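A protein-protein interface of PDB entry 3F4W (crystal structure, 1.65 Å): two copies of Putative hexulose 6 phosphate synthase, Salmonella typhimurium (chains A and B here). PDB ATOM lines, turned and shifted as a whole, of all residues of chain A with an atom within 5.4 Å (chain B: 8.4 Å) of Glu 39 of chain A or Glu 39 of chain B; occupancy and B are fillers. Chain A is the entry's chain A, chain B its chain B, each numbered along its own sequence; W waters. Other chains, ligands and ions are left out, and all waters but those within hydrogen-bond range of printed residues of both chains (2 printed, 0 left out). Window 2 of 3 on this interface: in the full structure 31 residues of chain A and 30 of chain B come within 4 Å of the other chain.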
ATOM      1  N   LEU A  12      12.204  -3.905  -4.212  1.00  0.00           N
ATOM      2  CA  LEU A  12      11.134  -4.901  -4.181  1.00  0.00           C
ATOM      3  C   LEU A  12      11.660  -6.333  -4.009  1.00  0.00           C
ATOM      4  O   LEU A  12      11.137  -7.085  -3.189  1.00  0.00           O
ATOM      5  CB  LEU A  12      10.231  -4.793  -5.415  1.00  0.00           C
ATOM      6  CG  LEU A  12       9.058  -5.775  -5.440  1.00  0.00           C
ATOM      7  CD1 LEU A  12       8.260  -5.716  -4.141  1.00  0.00           C
ATOM      8  CD2 LEU A  12       8.162  -5.510  -6.638  1.00  0.00           C
ATOM      9  N   PRO A  34      10.083   6.111   0.055  1.00  0.00           N
ATOM     10  CA  PRO A  34      11.150   5.931  -0.937  1.00  0.00           C
ATOM     11  C   PRO A  34      10.967   4.630  -1.713  1.00  0.00           C
ATOM     12  O   PRO A  34      11.349   4.533  -2.881  1.00  0.00           O
ATOM     13  CB  PRO A  34      12.414   5.856  -0.078  1.00  0.00           C
ATOM     14  CG  PRO A  34      12.060   6.547   1.191  1.00  0.00           C
ATOM     15  CD  PRO A  34      10.614   6.243   1.422  1.00  0.00           C
ATOM     16  N   PHE A  35      10.374   3.642  -1.056  1.00  0.00           N
ATOM     17  CA  PHE A  35      10.103   2.345  -1.667  1.00  0.00           C
ATOM     18  C   PHE A  35       9.047   2.525  -2.756  1.00  0.00           C
ATOM     19  O   PHE A  35       9.233   2.088  -3.896  1.00  0.00           O
ATOM     20  CB  PHE A  35       9.653   1.357  -0.578  1.00  0.00           C
ATOM     21  CG  PHE A  35       9.492  -0.063  -1.044  1.00  0.00           C
ATOM     22  CD1 PHE A  35       9.898  -0.458  -2.307  1.00  0.00           C
ATOM     23  CD2 PHE A  35       8.957  -1.020  -0.190  1.00  0.00           C
ATOM     24  CE1 PHE A  35       9.750  -1.776  -2.720  1.00  0.00           C
ATOM     25  CE2 PHE A  35       8.806  -2.334  -0.594  1.00  0.00           C
ATOM     26  CZ  PHE A  35       9.204  -2.714  -1.861  1.00  0.00           C
ATOM     27  N   LEU A  36       7.947   3.189  -2.405  1.00  0.00           N
ATOM     28  CA  LEU A  36       6.917   3.550  -3.376  1.00  0.00           C
ATOM     29  C   LEU A  36       7.492   4.332  -4.552  1.00  0.00           C
ATOM     30  O   LEU A  36       7.190   4.047  -5.708  1.00  0.00           O
ATOM     31  CB  LEU A  36       5.837   4.407  -2.721  1.00  0.00           C
ATOM     32  CG  LEU A  36       4.515   3.768  -2.320  1.00  0.00           C
ATOM     33  CD1 LEU A  36       3.587   4.849  -1.787  1.00  0.00           C
ATOM     34  CD2 LEU A  36       3.891   3.053  -3.505  1.00  0.00           C
ATOM     35  N   ILE A  37       8.298   5.344  -4.250  1.00  0.00           N
ATOM     36  CA  ILE A  37       8.880   6.186  -5.288  1.00  0.00           C
ATOM     37  C   ILE A  37       9.819   5.378  -6.179  1.00  0.00           C
ATOM     38  O   ILE A  37       9.890   5.593  -7.393  1.00  0.00           O
ATOM     39  CB  ILE A  37       9.646   7.369  -4.675  1.00  0.00           C
ATOM     40  CG1 ILE A  37       8.683   8.276  -3.902  1.00  0.00           C
ATOM     41  CG2 ILE A  37      10.386   8.143  -5.749  1.00  0.00           C
ATOM     42  CD1 ILE A  37       7.546   8.821  -4.737  1.00  0.00           C
ATOM     43  N   ARG A  38      10.531   4.441  -5.567  1.00  0.00           N
ATOM     44  CA  ARG A  38      11.463   3.582  -6.284  1.00  0.00           C
ATOM     45  C   ARG A  38      10.738   2.682  -7.275  1.00  0.00           C
ATOM     46  O   ARG A  38      11.041   2.674  -8.469  1.00  0.00           O
ATOM     47  CB  ARG A  38      12.228   2.721  -5.282  1.00  0.00           C
ATOM     48  CG  ARG A  38      13.364   1.913  -5.860  1.00  0.00           C
ATOM     49  CD  ARG A  38      14.166   1.299  -4.725  1.00  0.00           C
ATOM     50  NE  ARG A  38      15.598   1.410  -4.968  1.00  0.00           N
ATOM     51  CZ  ARG A  38      16.500   1.602  -4.013  1.00  0.00           C
ATOM     52  NH1 ARG A  38      16.115   1.716  -2.748  1.00  0.00           N
ATOM     53  NH2 ARG A  38      17.786   1.691  -4.327  1.00  0.00           N
ATOM     54  N   GLU A  39       9.764   1.937  -6.765  1.00  0.00           N
ATOM     55  CA  GLU A  39       9.177   0.822  -7.493  1.00  0.00           C
ATOM     56  C   GLU A  39       7.832   1.160  -8.129  1.00  0.00           C
ATOM     57  O   GLU A  39       7.416   0.528  -9.102  1.00  0.00           O
ATOM     58  CB  GLU A  39       9.020  -0.375  -6.544  1.00  0.00           C
ATOM     59  CG  GLU A  39       8.338  -1.588  -7.154  1.00  0.00           C
ATOM     60  CD  GLU A  39       9.131  -2.196  -8.292  1.00  0.00           C
ATOM     61  OE1 GLU A  39      10.370  -2.027  -8.320  1.00  0.00           O
ATOM     62  OE2 GLU A  39       8.511  -2.851  -9.155  1.00  0.00           O
ATOM     63  N   GLY A  40       7.151   2.155  -7.575  1.00  0.00           N
ATOM     64  CA  GLY A  40       5.802   2.462  -7.998  1.00  0.00           C
ATOM     65  C   GLY A  40       4.782   1.509  -7.405  1.00  0.00           C
ATOM     66  O   GLY A  40       5.097   0.685  -6.540  1.00  0.00           O
ATOM     67  N   VAL A  41       3.550   1.624  -7.884  1.00  0.00           N
ATOM     68  CA  VAL A  41       2.428   0.857  -7.355  1.00  0.00           C
ATOM     69  C   VAL A  41       2.631  -0.660  -7.450  1.00  0.00           C
ATOM     70  O   VAL A  41       1.989  -1.433  -6.736  1.00  0.00           O
ATOM     71  CB  VAL A  41       1.117   1.279  -8.057  1.00  0.00           C
ATOM     72  CG1 VAL A  41       0.225   0.084  -8.305  1.00  0.00           C
ATOM     73  CG2 VAL A  41       0.406   2.351  -7.243  1.00  0.00           C
ATOM     74  N   ASN A  42       3.535  -1.092  -8.321  1.00  0.00           N
ATOM     75  CA  ASN A  42       3.825  -2.515  -8.433  1.00  0.00           C
ATOM     76  C   ASN A  42       4.284  -3.126  -7.109  1.00  0.00           C
ATOM     77  O   ASN A  42       4.088  -4.315  -6.867  1.00  0.00           O
ATOM     78  CB  ASN A  42       4.864  -2.777  -9.516  1.00  0.00           C
ATOM     79  CG  ASN A  42       5.156  -4.249  -9.678  1.00  0.00           C
ATOM     80  OD1 ASN A  42       6.295  -4.689  -9.527  1.00  0.00           O
ATOM     81  ND2 ASN A  42       4.118  -5.028  -9.954  1.00  0.00           N
ATOM     82  N   ALA A  43       4.901  -2.310  -6.259  1.00  0.00           N
ATOM     83  CA  ALA A  43       5.346  -2.777  -4.950  1.00  0.00           C
ATOM     84  C   ALA A  43       4.161  -3.244  -4.108  1.00  0.00           C
ATOM     85  O   ALA A  43       4.212  -4.301  -3.482  1.00  0.00           O
ATOM     86  CB  ALA A  43       6.114  -1.685  -4.230  1.00  0.00           C
ATOM     87  N   LEU B  10      -1.030  11.041 -16.071  1.00  0.00           N
ATOM     88  CA  LEU B  10      -0.754  10.190 -17.223  1.00  0.00           C
ATOM     89  C   LEU B  10       0.031   8.951 -16.821  1.00  0.00           C
ATOM     90  O   LEU B  10       0.788   8.974 -15.852  1.00  0.00           O
ATOM     91  CB  LEU B  10       0.035  10.958 -18.288  1.00  0.00           C
ATOM     92  CG  LEU B  10      -0.635  12.155 -18.968  1.00  0.00           C
ATOM     93  CD1 LEU B  10       0.322  12.806 -19.955  1.00  0.00           C
ATOM     94  CD2 LEU B  10      -1.911  11.716 -19.664  1.00  0.00           C
ATOM     95  N   THR B  11      -0.152   7.869 -17.568  1.00  0.00           N
ATOM     96  CA  THR B  11       0.716   6.711 -17.440  1.00  0.00           C
ATOM     97  C   THR B  11       1.977   6.985 -18.248  1.00  0.00           C
ATOM     98  O   THR B  11       1.991   7.889 -19.085  1.00  0.00           O
ATOM     99  CB  THR B  11       0.052   5.448 -18.002  1.00  0.00           C
ATOM    100  OG1 THR B  11      -0.107   5.585 -19.420  1.00  0.00           O
ATOM    101  CG2 THR B  11      -1.307   5.229 -17.355  1.00  0.00           C
ATOM    102  N   LEU B  12       3.033   6.214 -18.008  1.00  0.00           N
ATOM    103  CA  LEU B  12       4.278   6.396 -18.752  1.00  0.00           C
ATOM    104  C   LEU B  12       4.065   6.314 -20.270  1.00  0.00           C
ATOM    105  O   LEU B  12       4.572   7.152 -21.010  1.00  0.00           O
ATOM    106  CB  LEU B  12       5.333   5.377 -18.319  1.00  0.00           C
ATOM    107  CG  LEU B  12       6.794   5.835 -18.275  1.00  0.00           C
ATOM    108  CD1 LEU B  12       7.717   4.684 -18.635  1.00  0.00           C
ATOM    109  CD2 LEU B  12       7.054   7.027 -19.178  1.00  0.00           C
ATOM    110  N   PRO B  13       3.326   5.296 -20.742  1.00  0.00           N
ATOM    111  CA  PRO B  13       3.111   5.229 -22.194  1.00  0.00           C
ATOM    112  C   PRO B  13       2.332   6.433 -22.715  1.00  0.00           C
ATOM    113  O   PRO B  13       2.605   6.914 -23.819  1.00  0.00           O
ATOM    114  CB  PRO B  13       2.302   3.938 -22.375  1.00  0.00           C
ATOM    115  CG  PRO B  13       2.645   3.108 -21.169  1.00  0.00           C
ATOM    116  CD  PRO B  13       2.817   4.097 -20.050  1.00  0.00           C
ATOM    117  N   GLU B  14       1.378   6.918 -21.927  1.00  0.00           N
ATOM    118  CA  GLU B  14       0.611   8.097 -22.312  1.00  0.00           C
ATOM    119  C   GLU B  14       1.503   9.332 -22.333  1.00  0.00           C
ATOM    120  O   GLU B  14       1.395  10.171 -23.225  1.00  0.00           O
ATOM    121  CB  GLU B  14      -0.569   8.314 -21.364  1.00  0.00           C
ATOM    122  CG  GLU B  14      -1.655   7.260 -21.482  1.00  0.00           C
ATOM    123  CD  GLU B  14      -2.759   7.432 -20.453  1.00  0.00           C
ATOM    124  OE1 GLU B  14      -3.862   6.889 -20.674  1.00  0.00           O
ATOM    125  OE2 GLU B  14      -2.530   8.110 -19.428  1.00  0.00           O
ATOM    126  N   ALA B  15       2.390   9.431 -21.349  1.00  0.00           N
ATOM    127  CA  ALA B  15       3.300  10.567 -21.243  1.00  0.00           C
ATOM    128  C   ALA B  15       4.271  10.624 -22.418  1.00  0.00           C
ATOM    129  O   ALA B  15       4.523  11.694 -22.971  1.00  0.00           O
ATOM    130  CB  ALA B  15       4.066  10.516 -19.921  1.00  0.00           C
ATOM    131  N   VAL B  31       7.732  15.214 -13.914  1.00  0.00           N
ATOM    132  CA  VAL B  31       7.038  13.988 -13.551  1.00  0.00           C
ATOM    133  C   VAL B  31       6.273  14.256 -12.255  1.00  0.00           C
ATOM    134  O   VAL B  31       6.873  14.384 -11.187  1.00  0.00           O
ATOM    135  CB  VAL B  31       8.025  12.828 -13.365  1.00  0.00           C
ATOM    136  CG1 VAL B  31       7.301  11.566 -12.895  1.00  0.00           C
ATOM    137  CG2 VAL B  31       8.777  12.576 -14.660  1.00  0.00           C
ATOM    138  N   GLY B  32       4.952  14.365 -12.356  1.00  0.00           N
ATOM    139  CA  GLY B  32       4.122  14.698 -11.210  1.00  0.00           C
ATOM    140  C   GLY B  32       4.051  13.597 -10.167  1.00  0.00           C
ATOM    141  O   GLY B  32       4.372  12.444 -10.446  1.00  0.00           O
ATOM    142  N   THR B  33       3.615  13.956  -8.963  1.00  0.00           N
ATOM    143  CA  THR B  33       3.627  13.030  -7.830  1.00  0.00           C
ATOM    144  C   THR B  33       2.865  11.723  -8.071  1.00  0.00           C
ATOM    145  O   THR B  33       3.385  10.647  -7.793  1.00  0.00           O
ATOM    146  CB  THR B  33       3.099  13.706  -6.557  1.00  0.00           C
ATOM    147  OG1 THR B  33       3.769  14.959  -6.381  1.00  0.00           O
ATOM    148  CG2 THR B  33       3.348  12.825  -5.341  1.00  0.00           C
ATOM    149  N   PRO B  34       1.625  11.810  -8.575  1.00  0.00           N
ATOM    150  CA  PRO B  34       0.867  10.582  -8.841  1.00  0.00           C
ATOM    151  C   PRO B  34       1.537   9.741  -9.928  1.00  0.00           C
ATOM    152  O   PRO B  34       1.429   8.514  -9.926  1.00  0.00           O
ATOM    153  CB  PRO B  34      -0.482  11.105  -9.339  1.00  0.00           C
ATOM    154  CG  PRO B  34      -0.573  12.500  -8.823  1.00  0.00           C
ATOM    155  CD  PRO B  34       0.823  13.019  -8.826  1.00  0.00           C
ATOM    156  N   PHE B  35       2.220  10.414 -10.846  1.00  0.00           N
ATOM    157  CA  PHE B  35       2.936   9.765 -11.938  1.00  0.00           C
ATOM    158  C   PHE B  35       4.125   8.990 -11.369  1.00  0.00           C
ATOM    159  O   PHE B  35       4.311   7.807 -11.673  1.00  0.00           O
ATOM    160  CB  PHE B  35       3.368  10.833 -12.959  1.00  0.00           C
ATOM    161  CG  PHE B  35       3.980  10.283 -14.220  1.00  0.00           C
ATOM    162  CD1 PHE B  35       3.978   8.923 -14.486  1.00  0.00           C
ATOM    163  CD2 PHE B  35       4.530  11.144 -15.160  1.00  0.00           C
ATOM    164  CE1 PHE B  35       4.544   8.429 -15.652  1.00  0.00           C
ATOM    165  CE2 PHE B  35       5.094  10.658 -16.329  1.00  0.00           C
ATOM    166  CZ  PHE B  35       5.099   9.298 -16.576  1.00  0.00           C
ATOM    167  N   LEU B  36       4.912   9.656 -10.526  1.00  0.00           N
ATOM    168  CA  LEU B  36       5.996   9.000  -9.796  1.00  0.00           C
ATOM    169  C   LEU B  36       5.506   7.802  -8.989  1.00  0.00           C
ATOM    170  O   LEU B  36       6.120   6.739  -9.008  1.00  0.00           O
ATOM    171  CB  LEU B  36       6.675   9.979  -8.837  1.00  0.00           C
ATOM    172  CG  LEU B  36       8.017  10.584  -9.225  1.00  0.00           C
ATOM    173  CD1 LEU B  36       8.537  11.437  -8.076  1.00  0.00           C
ATOM    174  CD2 LEU B  36       9.015   9.498  -9.588  1.00  0.00           C
ATOM    175  N   ILE B  37       4.416   7.995  -8.253  1.00  0.00           N
ATOM    176  CA  ILE B  37       3.866   6.950  -7.397  1.00  0.00           C
ATOM    177  C   ILE B  37       3.387   5.770  -8.234  1.00  0.00           C
ATOM    178  O   ILE B  37       3.566   4.610  -7.864  1.00  0.00           O
ATOM    179  CB  ILE B  37       2.688   7.488  -6.552  1.00  0.00           C
ATOM    180  CG1 ILE B  37       3.172   8.572  -5.587  1.00  0.00           C
ATOM    181  CG2 ILE B  37       2.019   6.367  -5.783  1.00  0.00           C
ATOM    182  CD1 ILE B  37       4.096   8.062  -4.503  1.00  0.00           C
ATOM    183  N   ARG B  38       2.780   6.088  -9.372  1.00  0.00           N
ATOM    184  CA  ARG B  38       2.263   5.087 -10.293  1.00  0.00           C
ATOM    185  C   ARG B  38       3.373   4.234 -10.890  1.00  0.00           C
ATOM    186  O   ARG B  38       3.315   3.003 -10.864  1.00  0.00           O
ATOM    187  CB  ARG B  38       1.519   5.789 -11.427  1.00  0.00           C
ATOM    188  CG  ARG B  38       0.791   4.866 -12.375  1.00  0.00           C
ATOM    189  CD  ARG B  38       0.158   5.656 -13.505  1.00  0.00           C
ATOM    190  NE  ARG B  38      -1.198   5.194 -13.771  1.00  0.00           N
ATOM    191  CZ  ARG B  38      -2.288   5.927 -13.573  1.00  0.00           C
ATOM    192  NH1 ARG B  38      -2.184   7.170 -13.124  1.00  0.00           N
ATOM    193  NH2 ARG B  38      -3.484   5.421 -13.840  1.00  0.00           N
ATOM    194  N   GLU B  39       4.390   4.909 -11.413  1.00  0.00           N
ATOM    195  CA  GLU B  39       5.363   4.298 -12.305  1.00  0.00           C
ATOM    196  C   GLU B  39       6.681   3.994 -11.597  1.00  0.00           C
ATOM    197  O   GLU B  39       7.384   3.042 -11.945  1.00  0.00           O
ATOM    198  CB  GLU B  39       5.618   5.257 -13.473  1.00  0.00           C
ATOM    199  CG  GLU B  39       5.889   4.597 -14.802  1.00  0.00           C
ATOM    200  CD  GLU B  39       4.735   3.723 -15.270  1.00  0.00           C
ATOM    201  OE1 GLU B  39       3.636   4.258 -15.544  1.00  0.00           O
ATOM    202  OE2 GLU B  39       4.932   2.495 -15.363  1.00  0.00           O
ATOM    203  N   GLY B  40       7.019   4.813 -10.609  1.00  0.00           N
ATOM    204  CA  GLY B  40       8.306   4.717  -9.954  1.00  0.00           C
ATOM    205  C   GLY B  40       9.387   5.453 -10.725  1.00  0.00           C
ATOM    206  O   GLY B  40       9.113   6.126 -11.725  1.00  0.00           O
ATOM    207  N   VAL B  41      10.622   5.318 -10.256  1.00  0.00           N
ATOM    208  CA  VAL B  41      11.761   6.026 -10.837  1.00  0.00           C
ATOM    209  C   VAL B  41      11.963   5.748 -12.334  1.00  0.00           C
ATOM    210  O   VAL B  41      12.588   6.538 -13.049  1.00  0.00           O
ATOM    211  CB  VAL B  41      13.047   5.721 -10.038  1.00  0.00           C
ATOM    212  CG1 VAL B  41      14.222   5.460 -10.963  1.00  0.00           C
ATOM    213  CG2 VAL B  41      13.335   6.849  -9.052  1.00  0.00           C
ATOM    214  N   ASN B  42      11.421   4.634 -12.814  1.00  0.00           N
ATOM    215  CA  ASN B  42      11.515   4.327 -14.234  1.00  0.00           C
ATOM    216  C   ASN B  42      10.918   5.428 -15.111  1.00  0.00           C
ATOM    217  O   ASN B  42      11.354   5.629 -16.243  1.00  0.00           O
ATOM    218  CB  ASN B  42      10.859   2.990 -14.554  1.00  0.00           C
ATOM    219  CG  ASN B  42      10.969   2.636 -16.018  1.00  0.00           C
ATOM    220  OD1 ASN B  42       9.963   2.441 -16.698  1.00  0.00           O
ATOM    221  ND2 ASN B  42      12.198   2.580 -16.521  1.00  0.00           N
ATOM    222  N   ALA B  43       9.920   6.138 -14.591  1.00  0.00           N
ATOM    223  CA  ALA B  43       9.328   7.256 -15.322  1.00  0.00           C
ATOM    224  C   ALA B  43      10.375   8.327 -15.629  1.00  0.00           C
ATOM    225  O   ALA B  43      10.433   8.849 -16.744  1.00  0.00           O
ATOM    226  CB  ALA B  43       8.171   7.854 -14.538  1.00  0.00           C
ATOM    227  N   ILE B  44      11.195   8.649 -14.635  1.00  0.00           N
ATOM    228  CA  ILE B  44      12.276   9.613 -14.805  1.00  0.00           C
ATOM    229  C   ILE B  44      13.297   9.126 -15.830  1.00  0.00           C
ATOM    230  O   ILE B  44      13.689   9.870 -16.730  1.00  0.00           O
ATOM    231  CB  ILE B  44      13.003   9.893 -13.478  1.00  0.00           C
ATOM    232  CG1 ILE B  44      12.034  10.483 -12.450  1.00  0.00           C
ATOM    233  CG2 ILE B  44      14.170  10.849 -13.694  1.00  0.00           C
ATOM    234  CD1 ILE B  44      11.607  11.895 -12.767  1.00  0.00           C
ATOM    235  N   ALA B  46      13.005   6.829 -18.274  1.00  0.00           N
ATOM    236  CA  ALA B  46      12.454   6.723 -19.621  1.00  0.00           C
ATOM    237  C   ALA B  46      12.381   8.085 -20.303  1.00  0.00           C
ATOM    238  O   ALA B  46      12.752   8.233 -21.467  1.00  0.00           O
ATOM    239  CB  ALA B  46      11.079   6.084 -19.580  1.00  0.00           C
ATOM    240  N   ILE B  47      11.895   9.077 -19.567  1.00  0.00           N
ATOM    241  CA  ILE B  47      11.724  10.417 -20.112  1.00  0.00           C
ATOM    242  C   ILE B  47      13.063  11.110 -20.362  1.00  0.00           C
ATOM    243  O   ILE B  47      13.260  11.726 -21.409  1.00  0.00           O
ATOM    244  CB  ILE B  47      10.843  11.283 -19.192  1.00  0.00           C
ATOM    245  CG1 ILE B  47       9.390  10.807 -19.266  1.00  0.00           C
ATOM    246  CG2 ILE B  47      10.950  12.756 -19.575  1.00  0.00           C
ATOM    247  CD1 ILE B  47       8.481  11.436 -18.232  1.00  0.00           C
ATOM    248  N   LEU B  72      18.173   8.956  -4.828  1.00  0.00           N
ATOM    249  CA  LEU B  72      17.492   7.996  -5.691  1.00  0.00           C
ATOM    250  C   LEU B  72      16.956   8.684  -6.945  1.00  0.00           C
ATOM    251  O   LEU B  72      17.109   8.185  -8.061  1.00  0.00           O
ATOM    252  CB  LEU B  72      16.342   7.341  -4.931  1.00  0.00           C
ATOM    253  CG  LEU B  72      15.413   6.452  -5.747  1.00  0.00           C
ATOM    254  CD1 LEU B  72      16.109   5.146  -6.084  1.00  0.00           C
ATOM    255  CD2 LEU B  72      14.138   6.196  -4.973  1.00  0.00           C
HETATM  256  O   HOH W   1       4.797   0.343 -10.454  1.00  0.00           O
HETATM  257  O   HOH W   2      10.223   2.396 -11.374  1.00  0.00           O
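The side-chain carboxylate (OE2) of Glu 39 of chain A lies close to the side-chain amide oxygen (OD1) of Asn 42 of chain A (2.9 Å).
The backbone NH of Leu 12 of chain B is in hydrogen-bond range of the side-chain carboxylate of Glu 39 of chain B, 3.2 Å away.
Pro 34 of chain A touches Leu 72 of chain B (O to CD2, 3.9 Å).
Ile 37 of chain B touches Ile 37 of chain A.
Gly 40 of chain B touches Ile 37 of chain A (CA to O, 3.1 Å).
Arg 38 of chain A touches Gly 40 of chain B (O to CA, 3.7 Å).
Arg 38 of chain A touches Leu 72 of chain B.
Glu 39 of chain A touches Glu 39 of chain B (O to O, 3.8 Å).
CA of Gly 40 of chain A touches O of Ile 37 of chain B, 3.1 Å away.
Gly 40 of chain A touches Arg 38 of chain B.
Gly 40 of chain A touches Gly 40 of chain B (N to CA, 3.7 Å).
The backbone NH (N) of Val 41 of chain B is in hydrogen-bond range of the backbone carbonyl oxygen (O) of Ile 37 of chain A (3.0 Å).
O of Arg 38 of chain A lies within hydrogen-bond range of N of Val 41 of chain B, at 3.2 Å.
The backbone carbonyl oxygen (O) of Ile 37 of chain B sits at hydrogen-bond distance from the backbone NH (N) of Val 41 of chain A (3.0 Å).
N of Val 41 of chain A is in hydrogen-bond range of O of Arg 38 of chain B (3.3 Å).
Of the 23 printed residues of chain B, 6 touch a printed residue of chain A.
Printed residues of chain B that touch a printed residue of chain A: Ile 37, Arg 38, Glu 39, Gly 40, Val 41 and Leu 72.
Of the 11 printed residues of chain A, 6 touch a printed residue of chain B.
Hydrophobic or aromatic side chains of chain A that line the printed part of chain B: Ile 37 and Val 41.
Among the printed residues, 13 pairs touch across the chains.
Among the printed residues, no Asp or Glu carboxylate lies within 4 Å of a Lys or Arg side-chain nitrogen of the other chain.
Of the printed residues of chain B, Pro 34 of chain A touches Leu 72 (3.9 Å).
Printed residues of chain B within 4 Å of Arg 38 of chain A: Gly 40, Val 41 and Leu 72.
Of chain B, only Glu 39 (3.8 Å) comes within 4 Å of Glu 39 of chain A.
Pro 13 of chain B touches none of the printed residues of chain A.
Of the printed residues of chain A, Arg 38 of chain B touches Gly 40 (3.8 Å) and Val 41 (3.3 Å).
Printed residues of chain A within 4 Å of Glu 39 of chain B: Glu 39 (3.8 Å).
Of the printed residues of chain A, Leu 72 of chain B touches Pro 34 (3.9 Å) and Arg 38 (3.9 Å).
The nearest residue of chain B that does not touch Glu 39 of chain A is Gly 40 of chain B (4.03 Å).
Ile 37 of chain A touches Gly 40 of chain B, and with the chains exchanged Gly 40 of chain A touches Ile 37 of chain B.
Ile 37 of chain A touches Val 41 of chain B, and with the chains exchanged Val 41 of chain A touches Ile 37 of chain B.
Arg 38 of chain A touches Val 41 of chain B, and with the chains exchanged Val 41 of chain A touches Arg 38 of chain B.
Glu 39 of chain A touches its own counterpart, Glu 39 of chain B.
Positions printed for both chains: 12, 34, 35, 36, 37, 38, 39, 40, 41, 42 and 43.
Water W1 lies within hydrogen-bond range of N of Asn 42 of chain A (2.9 Å), O of Glu 39 of chain A (3.0 Å), O of Arg 38 of chain B (3.1 Å) and N of Val 41 of chain A (3.1 Å).
Water W2 lies within hydrogen-bond range of N of Asn 42 of chain B (2.9 Å), O of Glu 39 of chain B (3.0 Å), O of Arg 38 of chain A (3.0 Å) and N of Val 41 of chain B (3.2 Å).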
